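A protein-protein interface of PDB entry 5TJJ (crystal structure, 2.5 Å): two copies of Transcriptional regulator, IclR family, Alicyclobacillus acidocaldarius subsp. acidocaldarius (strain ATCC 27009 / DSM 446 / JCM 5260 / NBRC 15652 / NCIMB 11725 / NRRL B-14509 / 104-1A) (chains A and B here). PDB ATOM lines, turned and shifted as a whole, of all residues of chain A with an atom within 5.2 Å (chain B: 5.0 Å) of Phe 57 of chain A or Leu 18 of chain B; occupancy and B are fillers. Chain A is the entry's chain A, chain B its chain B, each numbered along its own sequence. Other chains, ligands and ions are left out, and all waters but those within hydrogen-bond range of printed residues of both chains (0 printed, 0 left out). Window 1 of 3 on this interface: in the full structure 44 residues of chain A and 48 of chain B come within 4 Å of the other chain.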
ATOM      1  N   LEU A  18       8.026  29.777  13.200  1.00  0.00           N
ATOM      2  CA  LEU A  18       8.297  28.479  13.788  1.00  0.00           C
ATOM      3  C   LEU A  18       9.704  28.001  13.501  1.00  0.00           C
ATOM      4  O   LEU A  18      10.348  27.393  14.367  1.00  0.00           O
ATOM      5  CB  LEU A  18       7.281  27.452  13.329  1.00  0.00           C
ATOM      6  CG  LEU A  18       5.844  27.745  13.766  1.00  0.00           C
ATOM      7  CD1 LEU A  18       4.887  26.800  13.053  1.00  0.00           C
ATOM      8  CD2 LEU A  18       5.700  27.607  15.274  1.00  0.00           C
ATOM      9  N   LEU A  52      -1.240  31.079  16.358  1.00  0.00           N
ATOM     10  CA  LEU A  52      -0.483  29.839  16.580  1.00  0.00           C
ATOM     11  C   LEU A  52      -0.620  29.312  18.011  1.00  0.00           C
ATOM     12  O   LEU A  52      -0.765  28.111  18.223  1.00  0.00           O
ATOM     13  CB  LEU A  52       1.015  30.027  16.233  1.00  0.00           C
ATOM     14  CG  LEU A  52       1.399  30.331  14.774  1.00  0.00           C
ATOM     15  CD1 LEU A  52       2.879  30.632  14.636  1.00  0.00           C
ATOM     16  CD2 LEU A  52       1.035  29.212  13.831  1.00  0.00           C
ATOM     17  N   GLU A  53      -0.576  30.215  18.983  1.00  0.00           N
ATOM     18  CA  GLU A  53      -0.749  29.869  20.395  1.00  0.00           C
ATOM     19  C   GLU A  53      -2.115  29.252  20.690  1.00  0.00           C
ATOM     20  O   GLU A  53      -2.231  28.347  21.513  1.00  0.00           O
ATOM     21  CB  GLU A  53      -0.551  31.107  21.280  1.00  0.00           C
ATOM     22  CG  GLU A  53      -0.178  30.770  22.717  1.00  0.00           C
ATOM     23  CD  GLU A  53      -0.612  31.826  23.733  1.00  0.00           C
ATOM     24  OE1 GLU A  53      -1.292  31.433  24.709  1.00  0.00           O
ATOM     25  OE2 GLU A  53      -0.263  33.033  23.574  1.00  0.00           O
ATOM     26  N   GLU A  55      -3.881  27.415  18.705  1.00  0.00           N
ATOM     27  CA  GLU A  55      -3.857  26.043  18.202  1.00  0.00           C
ATOM     28  C   GLU A  55      -2.777  25.178  18.871  1.00  0.00           C
ATOM     29  O   GLU A  55      -2.633  24.018  18.491  1.00  0.00           O
ATOM     30  CB  GLU A  55      -3.650  26.037  16.673  1.00  0.00           C
ATOM     31  CG  GLU A  55      -4.593  26.940  15.852  1.00  0.00           C
ATOM     32  CD  GLU A  55      -5.959  26.315  15.502  1.00  0.00           C
ATOM     33  OE1 GLU A  55      -6.286  25.182  15.978  1.00  0.00           O
ATOM     34  OE2 GLU A  55      -6.718  26.972  14.724  1.00  0.00           O
ATOM     35  N   ASP A  56      -2.038  25.725  19.851  1.00  0.00           N
ATOM     36  CA  ASP A  56      -0.980  25.024  20.604  1.00  0.00           C
ATOM     37  C   ASP A  56       0.286  24.689  19.744  1.00  0.00           C
ATOM     38  O   ASP A  56       1.076  23.797  20.096  1.00  0.00           O
ATOM     39  CB  ASP A  56      -1.538  23.780  21.330  1.00  0.00           C
ATOM     40  CG  ASP A  56      -2.649  24.123  22.389  1.00  0.00           C
ATOM     41  OD1 ASP A  56      -2.259  24.548  23.493  1.00  0.00           O
ATOM     42  OD2 ASP A  56      -3.897  23.956  22.147  1.00  0.00           O
ATOM     43  N   PHE A  57       0.480  25.409  18.631  1.00  0.00           N
ATOM     44  CA  PHE A  57       1.691  25.313  17.821  1.00  0.00           C
ATOM     45  C   PHE A  57       2.820  26.204  18.382  1.00  0.00           C
ATOM     46  O   PHE A  57       4.000  25.996  18.068  1.00  0.00           O
ATOM     47  CB  PHE A  57       1.415  25.736  16.378  1.00  0.00           C
ATOM     48  CG  PHE A  57       0.681  24.706  15.535  1.00  0.00           C
ATOM     49  CD1 PHE A  57      -0.119  23.712  16.085  1.00  0.00           C
ATOM     50  CD2 PHE A  57       0.729  24.803  14.149  1.00  0.00           C
ATOM     51  CE1 PHE A  57      -0.812  22.813  15.262  1.00  0.00           C
ATOM     52  CE2 PHE A  57       0.037  23.905  13.327  1.00  0.00           C
ATOM     53  CZ  PHE A  57      -0.730  22.904  13.881  1.00  0.00           C
ATOM     54  N   VAL A  58       2.446  27.192  19.203  1.00  0.00           N
ATOM     55  CA  VAL A  58       3.378  28.058  19.940  1.00  0.00           C
ATOM     56  C   VAL A  58       2.924  28.100  21.391  1.00  0.00           C
ATOM     57  O   VAL A  58       1.740  27.934  21.663  1.00  0.00           O
ATOM     58  CB  VAL A  58       3.390  29.485  19.311  1.00  0.00           C
ATOM     59  CG1 VAL A  58       3.873  30.551  20.288  1.00  0.00           C
ATOM     60  CG2 VAL A  58       4.237  29.489  18.033  1.00  0.00           C
ATOM     61  N   SER A  59       3.838  28.312  22.333  1.00  0.00           N
ATOM     62  CA  SER A  59       3.413  28.702  23.694  1.00  0.00           C
ATOM     63  C   SER A  59       4.025  29.999  24.138  1.00  0.00           C
ATOM     64  O   SER A  59       4.999  30.479  23.579  1.00  0.00           O
ATOM     65  CB  SER A  59       3.637  27.602  24.741  1.00  0.00           C
ATOM     66  OG  SER A  59       4.729  26.786  24.413  1.00  0.00           O
ATOM     67  N   SER A  68       7.710  30.233  22.444  1.00  0.00           N
ATOM     68  CA  SER A  68       8.496  29.060  22.142  1.00  0.00           C
ATOM     69  C   SER A  68       7.665  28.092  21.355  1.00  0.00           C
ATOM     70  O   SER A  68       6.431  28.233  21.295  1.00  0.00           O
ATOM     71  CB  SER A  68       8.948  28.389  23.433  1.00  0.00           C
ATOM     72  OG  SER A  68       7.832  28.188  24.280  1.00  0.00           O
ATOM     73  N   LEU A  69       8.350  27.123  20.745  1.00  0.00           N
ATOM     74  CA  LEU A  69       7.658  26.041  20.043  1.00  0.00           C
ATOM     75  C   LEU A  69       6.652  25.340  20.945  1.00  0.00           C
ATOM     76  O   LEU A  69       7.001  24.889  22.022  1.00  0.00           O
ATOM     77  CB  LEU A  69       8.643  25.018  19.497  1.00  0.00           C
ATOM     78  CG  LEU A  69       9.537  25.504  18.348  1.00  0.00           C
ATOM     79  CD1 LEU A  69      10.367  24.361  17.791  1.00  0.00           C
ATOM     80  CD2 LEU A  69       8.727  26.142  17.225  1.00  0.00           C
ATOM     81  N   GLY A  70       5.402  25.256  20.487  1.00  0.00           N
ATOM     82  CA  GLY A  70       4.332  24.622  21.252  1.00  0.00           C
ATOM     83  C   GLY A  70       4.293  23.101  21.109  1.00  0.00           C
ATOM     84  O   GLY A  70       4.886  22.553  20.177  1.00  0.00           O
ATOM     85  N   TYR A  72       1.991  20.811  20.181  1.00  0.00           N
ATOM     86  CA  TYR A  72       1.302  20.126  19.087  1.00  0.00           C
ATOM     87  C   TYR A  72       2.274  19.725  17.968  1.00  0.00           C
ATOM     88  O   TYR A  72       2.055  18.732  17.267  1.00  0.00           O
ATOM     89  CB  TYR A  72       0.153  20.988  18.495  1.00  0.00           C
ATOM     90  CG  TYR A  72      -1.042  20.179  18.094  1.00  0.00           C
ATOM     91  CD1 TYR A  72      -0.969  19.262  17.041  1.00  0.00           C
ATOM     92  CD2 TYR A  72      -2.241  20.291  18.787  1.00  0.00           C
ATOM     93  CE1 TYR A  72      -2.064  18.489  16.685  1.00  0.00           C
ATOM     94  CE2 TYR A  72      -3.348  19.527  18.437  1.00  0.00           C
ATOM     95  CZ  TYR A  72      -3.253  18.632  17.384  1.00  0.00           C
ATOM     96  OH  TYR A  72      -4.338  17.867  17.038  1.00  0.00           O
ATOM     97  N   LEU A  73       3.371  20.457  17.825  1.00  0.00           N
ATOM     98  CA  LEU A  73       4.385  20.110  16.821  1.00  0.00           C
ATOM     99  C   LEU A  73       5.066  18.742  17.085  1.00  0.00           C
ATOM    100  O   LEU A  73       5.587  18.114  16.169  1.00  0.00           O
ATOM    101  CB  LEU A  73       5.423  21.237  16.725  1.00  0.00           C
ATOM    102  CG  LEU A  73       4.817  22.619  16.403  1.00  0.00           C
ATOM    103  CD1 LEU A  73       5.856  23.715  16.509  1.00  0.00           C
ATOM    104  CD2 LEU A  73       4.147  22.616  15.040  1.00  0.00           C
ATOM    105  N   LEU A  76       2.742  15.967  15.492  1.00  0.00           N
ATOM    106  CA  LEU A  76       2.852  16.216  14.035  1.00  0.00           C
ATOM    107  C   LEU A  76       4.117  15.697  13.424  1.00  0.00           C
ATOM    108  O   LEU A  76       4.077  15.079  12.367  1.00  0.00           O
ATOM    109  CB  LEU A  76       2.787  17.705  13.715  1.00  0.00           C
ATOM    110  CG  LEU A  76       1.444  18.370  13.933  1.00  0.00           C
ATOM    111  CD1 LEU A  76       1.534  19.762  13.356  1.00  0.00           C
ATOM    112  CD2 LEU A  76       0.317  17.588  13.295  1.00  0.00           C
ATOM    113  N   ALA B  14      -4.436  26.870   8.137  1.00  0.00           N
ATOM    114  CA  ALA B  14      -3.192  26.062   8.012  1.00  0.00           C
ATOM    115  C   ALA B  14      -3.052  25.017   9.128  1.00  0.00           C
ATOM    116  O   ALA B  14      -2.730  23.879   8.874  1.00  0.00           O
ATOM    117  CB  ALA B  14      -1.954  26.963   7.971  1.00  0.00           C
ATOM    118  N   ALA B  15      -3.317  25.434  10.355  1.00  0.00           N
ATOM    119  CA  ALA B  15      -3.310  24.552  11.525  1.00  0.00           C
ATOM    120  C   ALA B  15      -4.346  23.449  11.427  1.00  0.00           C
ATOM    121  O   ALA B  15      -4.063  22.321  11.755  1.00  0.00           O
ATOM    122  CB  ALA B  15      -3.579  25.363  12.791  1.00  0.00           C
ATOM    123  N   ARG B  16      -5.579  23.791  11.050  1.00  0.00           N
ATOM    124  CA  ARG B  16      -6.628  22.784  10.907  1.00  0.00           C
ATOM    125  C   ARG B  16      -6.245  21.743   9.840  1.00  0.00           C
ATOM    126  O   ARG B  16      -6.531  20.563  10.000  1.00  0.00           O
ATOM    127  CB  ARG B  16      -7.965  23.436  10.529  1.00  0.00           C
ATOM    128  CG  ARG B  16      -8.594  24.227  11.636  1.00  0.00           C
ATOM    129  CD  ARG B  16      -9.860  24.882  11.156  1.00  0.00           C
ATOM    130  NE  ARG B  16     -10.964  23.929  10.955  1.00  0.00           N
ATOM    131  CZ  ARG B  16     -12.020  24.117  10.140  1.00  0.00           C
ATOM    132  NH1 ARG B  16     -12.136  25.218   9.393  1.00  0.00           N
ATOM    133  NH2 ARG B  16     -12.949  23.173  10.052  1.00  0.00           N
ATOM    134  N   VAL B  17      -5.639  22.188   8.743  1.00  0.00           N
ATOM    135  CA  VAL B  17      -5.187  21.283   7.677  1.00  0.00           C
ATOM    136  C   VAL B  17      -4.181  20.302   8.248  1.00  0.00           C
ATOM    137  O   VAL B  17      -4.301  19.101   8.049  1.00  0.00           O
ATOM    138  CB  VAL B  17      -4.532  22.054   6.509  1.00  0.00           C
ATOM    139  CG1 VAL B  17      -3.767  21.120   5.601  1.00  0.00           C
ATOM    140  CG2 VAL B  17      -5.555  22.814   5.698  1.00  0.00           C
ATOM    141  N   LEU B  18      -3.180  20.822   8.950  1.00  0.00           N
ATOM    142  CA  LEU B  18      -2.138  19.982   9.524  1.00  0.00           C
ATOM    143  C   LEU B  18      -2.718  18.947  10.468  1.00  0.00           C
ATOM    144  O   LEU B  18      -2.306  17.777  10.448  1.00  0.00           O
ATOM    145  CB  LEU B  18      -1.061  20.828  10.232  1.00  0.00           C
ATOM    146  CG  LEU B  18      -0.142  21.629   9.291  1.00  0.00           C
ATOM    147  CD1 LEU B  18       0.912  22.410  10.069  1.00  0.00           C
ATOM    148  CD2 LEU B  18       0.557  20.741   8.276  1.00  0.00           C
ATOM    149  N   LYS B  19      -3.666  19.374  11.297  1.00  0.00           N
ATOM    150  CA  LYS B  19      -4.274  18.471  12.275  1.00  0.00           C
ATOM    151  C   LYS B  19      -5.078  17.380  11.578  1.00  0.00           C
ATOM    152  O   LYS B  19      -5.041  16.220  12.019  1.00  0.00           O
ATOM    153  CB  LYS B  19      -5.131  19.215  13.293  1.00  0.00           C
ATOM    154  CG  LYS B  19      -4.303  20.047  14.261  1.00  0.00           C
ATOM    155  CD  LYS B  19      -5.195  20.886  15.194  1.00  0.00           C
ATOM    156  CE  LYS B  19      -4.391  21.992  15.870  1.00  0.00           C
ATOM    157  NZ  LYS B  19      -5.062  22.688  17.018  1.00  0.00           N
ATOM    158  N   LEU B  20      -5.762  17.753  10.491  1.00  0.00           N
ATOM    159  CA  LEU B  20      -6.493  16.797   9.660  1.00  0.00           C
ATOM    160  C   LEU B  20      -5.562  15.758   9.045  1.00  0.00           C
ATOM    161  O   LEU B  20      -5.827  14.572   9.131  1.00  0.00           O
ATOM    162  CB  LEU B  20      -7.269  17.503   8.561  1.00  0.00           C
ATOM    163  CG  LEU B  20      -8.111  16.563   7.692  1.00  0.00           C
ATOM    164  CD1 LEU B  20      -9.174  15.833   8.509  1.00  0.00           C
ATOM    165  CD2 LEU B  20      -8.749  17.290   6.528  1.00  0.00           C
ATOM    166  N   LEU B  21      -4.458  16.209   8.457  1.00  0.00           N
ATOM    167  CA  LEU B  21      -3.486  15.301   7.834  1.00  0.00           C
ATOM    168  C   LEU B  21      -2.727  14.367   8.810  1.00  0.00           C
ATOM    169  O   LEU B  21      -2.123  13.395   8.350  1.00  0.00           O
ATOM    170  CB  LEU B  21      -2.482  16.086   6.985  1.00  0.00           C
ATOM    171  CG  LEU B  21      -3.028  16.849   5.772  1.00  0.00           C
ATOM    172  CD1 LEU B  21      -1.914  17.606   5.062  1.00  0.00           C
ATOM    173  CD2 LEU B  21      -3.765  15.928   4.819  1.00  0.00           C
ATOM    174  N   SER B  22      -2.779  14.632  10.120  1.00  0.00           N
ATOM    175  CA  SER B  22      -2.221  13.707  11.148  1.00  0.00           C
ATOM    176  C   SER B  22      -3.163  12.533  11.515  1.00  0.00           C
ATOM    177  O   SER B  22      -2.716  11.518  12.041  1.00  0.00           O
ATOM    178  CB  SER B  22      -1.796  14.473  12.425  1.00  0.00           C
ATOM    179  OG  SER B  22      -2.923  14.938  13.146  1.00  0.00           O
ATOM    180  N   LEU B  52       1.933  26.095   2.358  1.00  0.00           N
ATOM    181  CA  LEU B  52       2.470  25.094   3.235  1.00  0.00           C
ATOM    182  C   LEU B  52       3.409  24.137   2.519  1.00  0.00           C
ATOM    183  O   LEU B  52       4.372  23.678   3.123  1.00  0.00           O
ATOM    184  CB  LEU B  52       1.335  24.295   3.901  1.00  0.00           C
ATOM    185  CG  LEU B  52       0.559  24.991   5.029  1.00  0.00           C
ATOM    186  CD1 LEU B  52      -0.556  24.080   5.486  1.00  0.00           C
ATOM    187  CD2 LEU B  52       1.456  25.353   6.202  1.00  0.00           C
ATOM    188  N   PHE B  57       6.040  22.017   4.902  1.00  0.00           N
ATOM    189  CA  PHE B  57       5.125  21.608   5.994  1.00  0.00           C
ATOM    190  C   PHE B  57       4.122  20.586   5.507  1.00  0.00           C
ATOM    191  O   PHE B  57       3.549  19.851   6.294  1.00  0.00           O
ATOM    192  CB  PHE B  57       4.357  22.800   6.539  1.00  0.00           C
ATOM    193  CG  PHE B  57       5.126  23.617   7.504  1.00  0.00           C
ATOM    194  CD1 PHE B  57       6.447  23.940   7.280  1.00  0.00           C
ATOM    195  CD2 PHE B  57       4.506  24.116   8.634  1.00  0.00           C
ATOM    196  CE1 PHE B  57       7.149  24.720   8.176  1.00  0.00           C
ATOM    197  CE2 PHE B  57       5.206  24.908   9.542  1.00  0.00           C
ATOM    198  CZ  PHE B  57       6.535  25.201   9.320  1.00  0.00           C
ATOM    199  N   VAL B  58       3.917  20.570   4.200  1.00  0.00           N
ATOM    200  CA  VAL B  58       3.044  19.626   3.527  1.00  0.00           C
ATOM    201  C   VAL B  58       3.807  19.097   2.324  1.00  0.00           C
ATOM    202  O   VAL B  58       4.630  19.806   1.719  1.00  0.00           O
ATOM    203  CB  VAL B  58       1.761  20.379   3.122  1.00  0.00           C
ATOM    204  CG1 VAL B  58       1.150  19.872   1.864  1.00  0.00           C
ATOM    205  CG2 VAL B  58       0.736  20.351   4.264  1.00  0.00           C
ATOM    206  N   LEU B  69       1.394  15.256   5.490  1.00  0.00           N
ATOM    207  CA  LEU B  69       2.347  15.995   6.307  1.00  0.00           C
ATOM    208  C   LEU B  69       3.752  15.874   5.730  1.00  0.00           C
ATOM    209  O   LEU B  69       4.168  14.817   5.271  1.00  0.00           O
ATOM    210  CB  LEU B  69       2.365  15.493   7.741  1.00  0.00           C
ATOM    211  CG  LEU B  69       1.089  15.678   8.556  1.00  0.00           C
ATOM    212  CD1 LEU B  69       1.335  14.971   9.865  1.00  0.00           C
ATOM    213  CD2 LEU B  69       0.706  17.143   8.795  1.00  0.00           C
ATOM    214  N   LEU B  73       8.214  19.215   9.216  1.00  0.00           N
ATOM    215  CA  LEU B  73       7.673  18.972  10.550  1.00  0.00           C
ATOM    216  C   LEU B  73       8.532  18.026  11.419  1.00  0.00           C
ATOM    217  O   LEU B  73       8.379  18.013  12.629  1.00  0.00           O
ATOM    218  CB  LEU B  73       6.254  18.430  10.418  1.00  0.00           C
ATOM    219  CG  LEU B  73       5.308  19.347   9.650  1.00  0.00           C
ATOM    220  CD1 LEU B  73       4.046  18.577   9.362  1.00  0.00           C
ATOM    221  CD2 LEU B  73       5.035  20.634  10.409  1.00  0.00           C
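Hydrophobic or aromatic side chains of chain A that line the printed part of chain B: Phe 57, Tyr 72 and Leu 76.
Of the 14 printed residues of chain B, 5 touch a printed residue of chain A.
Printed residues of chain B that touch a printed residue of chain A: Ala 15, Leu 18, Lys 19, Ser 22 and Leu 69.
Among the printed residues, 9 pairs touch across the chains.
Among the printed residues, Asp or Glu carboxylates within 4 Å of a Lys or Arg side-chain nitrogen of the other chain: Glu 55 of chain A with Lys 19 of chain B.
The side-chain amino group (NZ) of Lys 19 of chain B lies within salt-bridge range of the side-chain carboxylate (OE1) of Glu 55 of chain A, 3.0 Å away.
N of Gly 70 of chain A lies within hydrogen-bond range of O of Phe 57 of chain A, at 2.9 Å.
The backbone carbonyl oxygen of Asp 56 of chain A sits at hydrogen-bond distance from the backbone NH of Tyr 72 of chain A (3.1 Å).
N of Phe 57 of chain A lies within hydrogen-bond range of O of Leu 52 of chain A (3.0 Å).
The side-chain hydroxyl (OG) of Ser 22 of chain B lies within hydrogen-bond range of the backbone carbonyl oxygen (O) of Lys 19 of chain B (2.7 Å).
Phe 57 of chain A touches Leu 18 of chain B, but with the chains exchanged Leu 18 of chain A does not touch Phe 57 of chain B (4.001 Å).
Positions printed for both chains: 18, 52, 57, 58, 69 and 73.
Of chain B, only Ala 15 (3.9 Å), Leu 18 (3.7 Å) and Lys 19 (3.7 Å) come within 4 Å of Phe 57 of chain A.
Of chain A, only Phe 57 and Leu 76 come within 4 Å of Leu 18 of chain B.
Of the printed residues of chain A, Ser 22 of chain B touches Leu 76.
Printed residues of chain B within 4 Å of Leu 76 of chain A: Leu 18, Ser 22 and Leu 69.
Of the printed residues of chain B, Glu 55 of chain A touches Ala 15 and Lys 19.
Printed residues of chain A within 4 Å of Lys 19 of chain B: Glu 55, Phe 57 and Tyr 72.
The nearest printed residue of chain B that does not touch Phe 57 of chain A is Ala 14 of chain B (5.2 Å).
The nearest printed residue of chain A that does not touch Leu 18 of chain B is Leu 73 of chain A (5.9 Å).
Among the printed residues, merely in contact across the chains: Tyr 72 of chain A with Lys 19 of chain B (3.5 Å), Glu 55 of chain A with Ala 15 of chain B (3.6 Å), Phe 57 of chain A with Leu 18 of chain B (3.7 Å), Leu 76 of chain A with Leu 69 of chain B (3.7 Å), Phe 57 of chain A with Lys 19 of chain B (3.7 Å), Phe 57 of chain A with Ala 15 of chain B (3.9 Å), Leu 76 of chain A with Ser 22 of chain B (3.9 Å) and Leu 76 of chain A with Leu 18 of chain B (3.9 Å).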
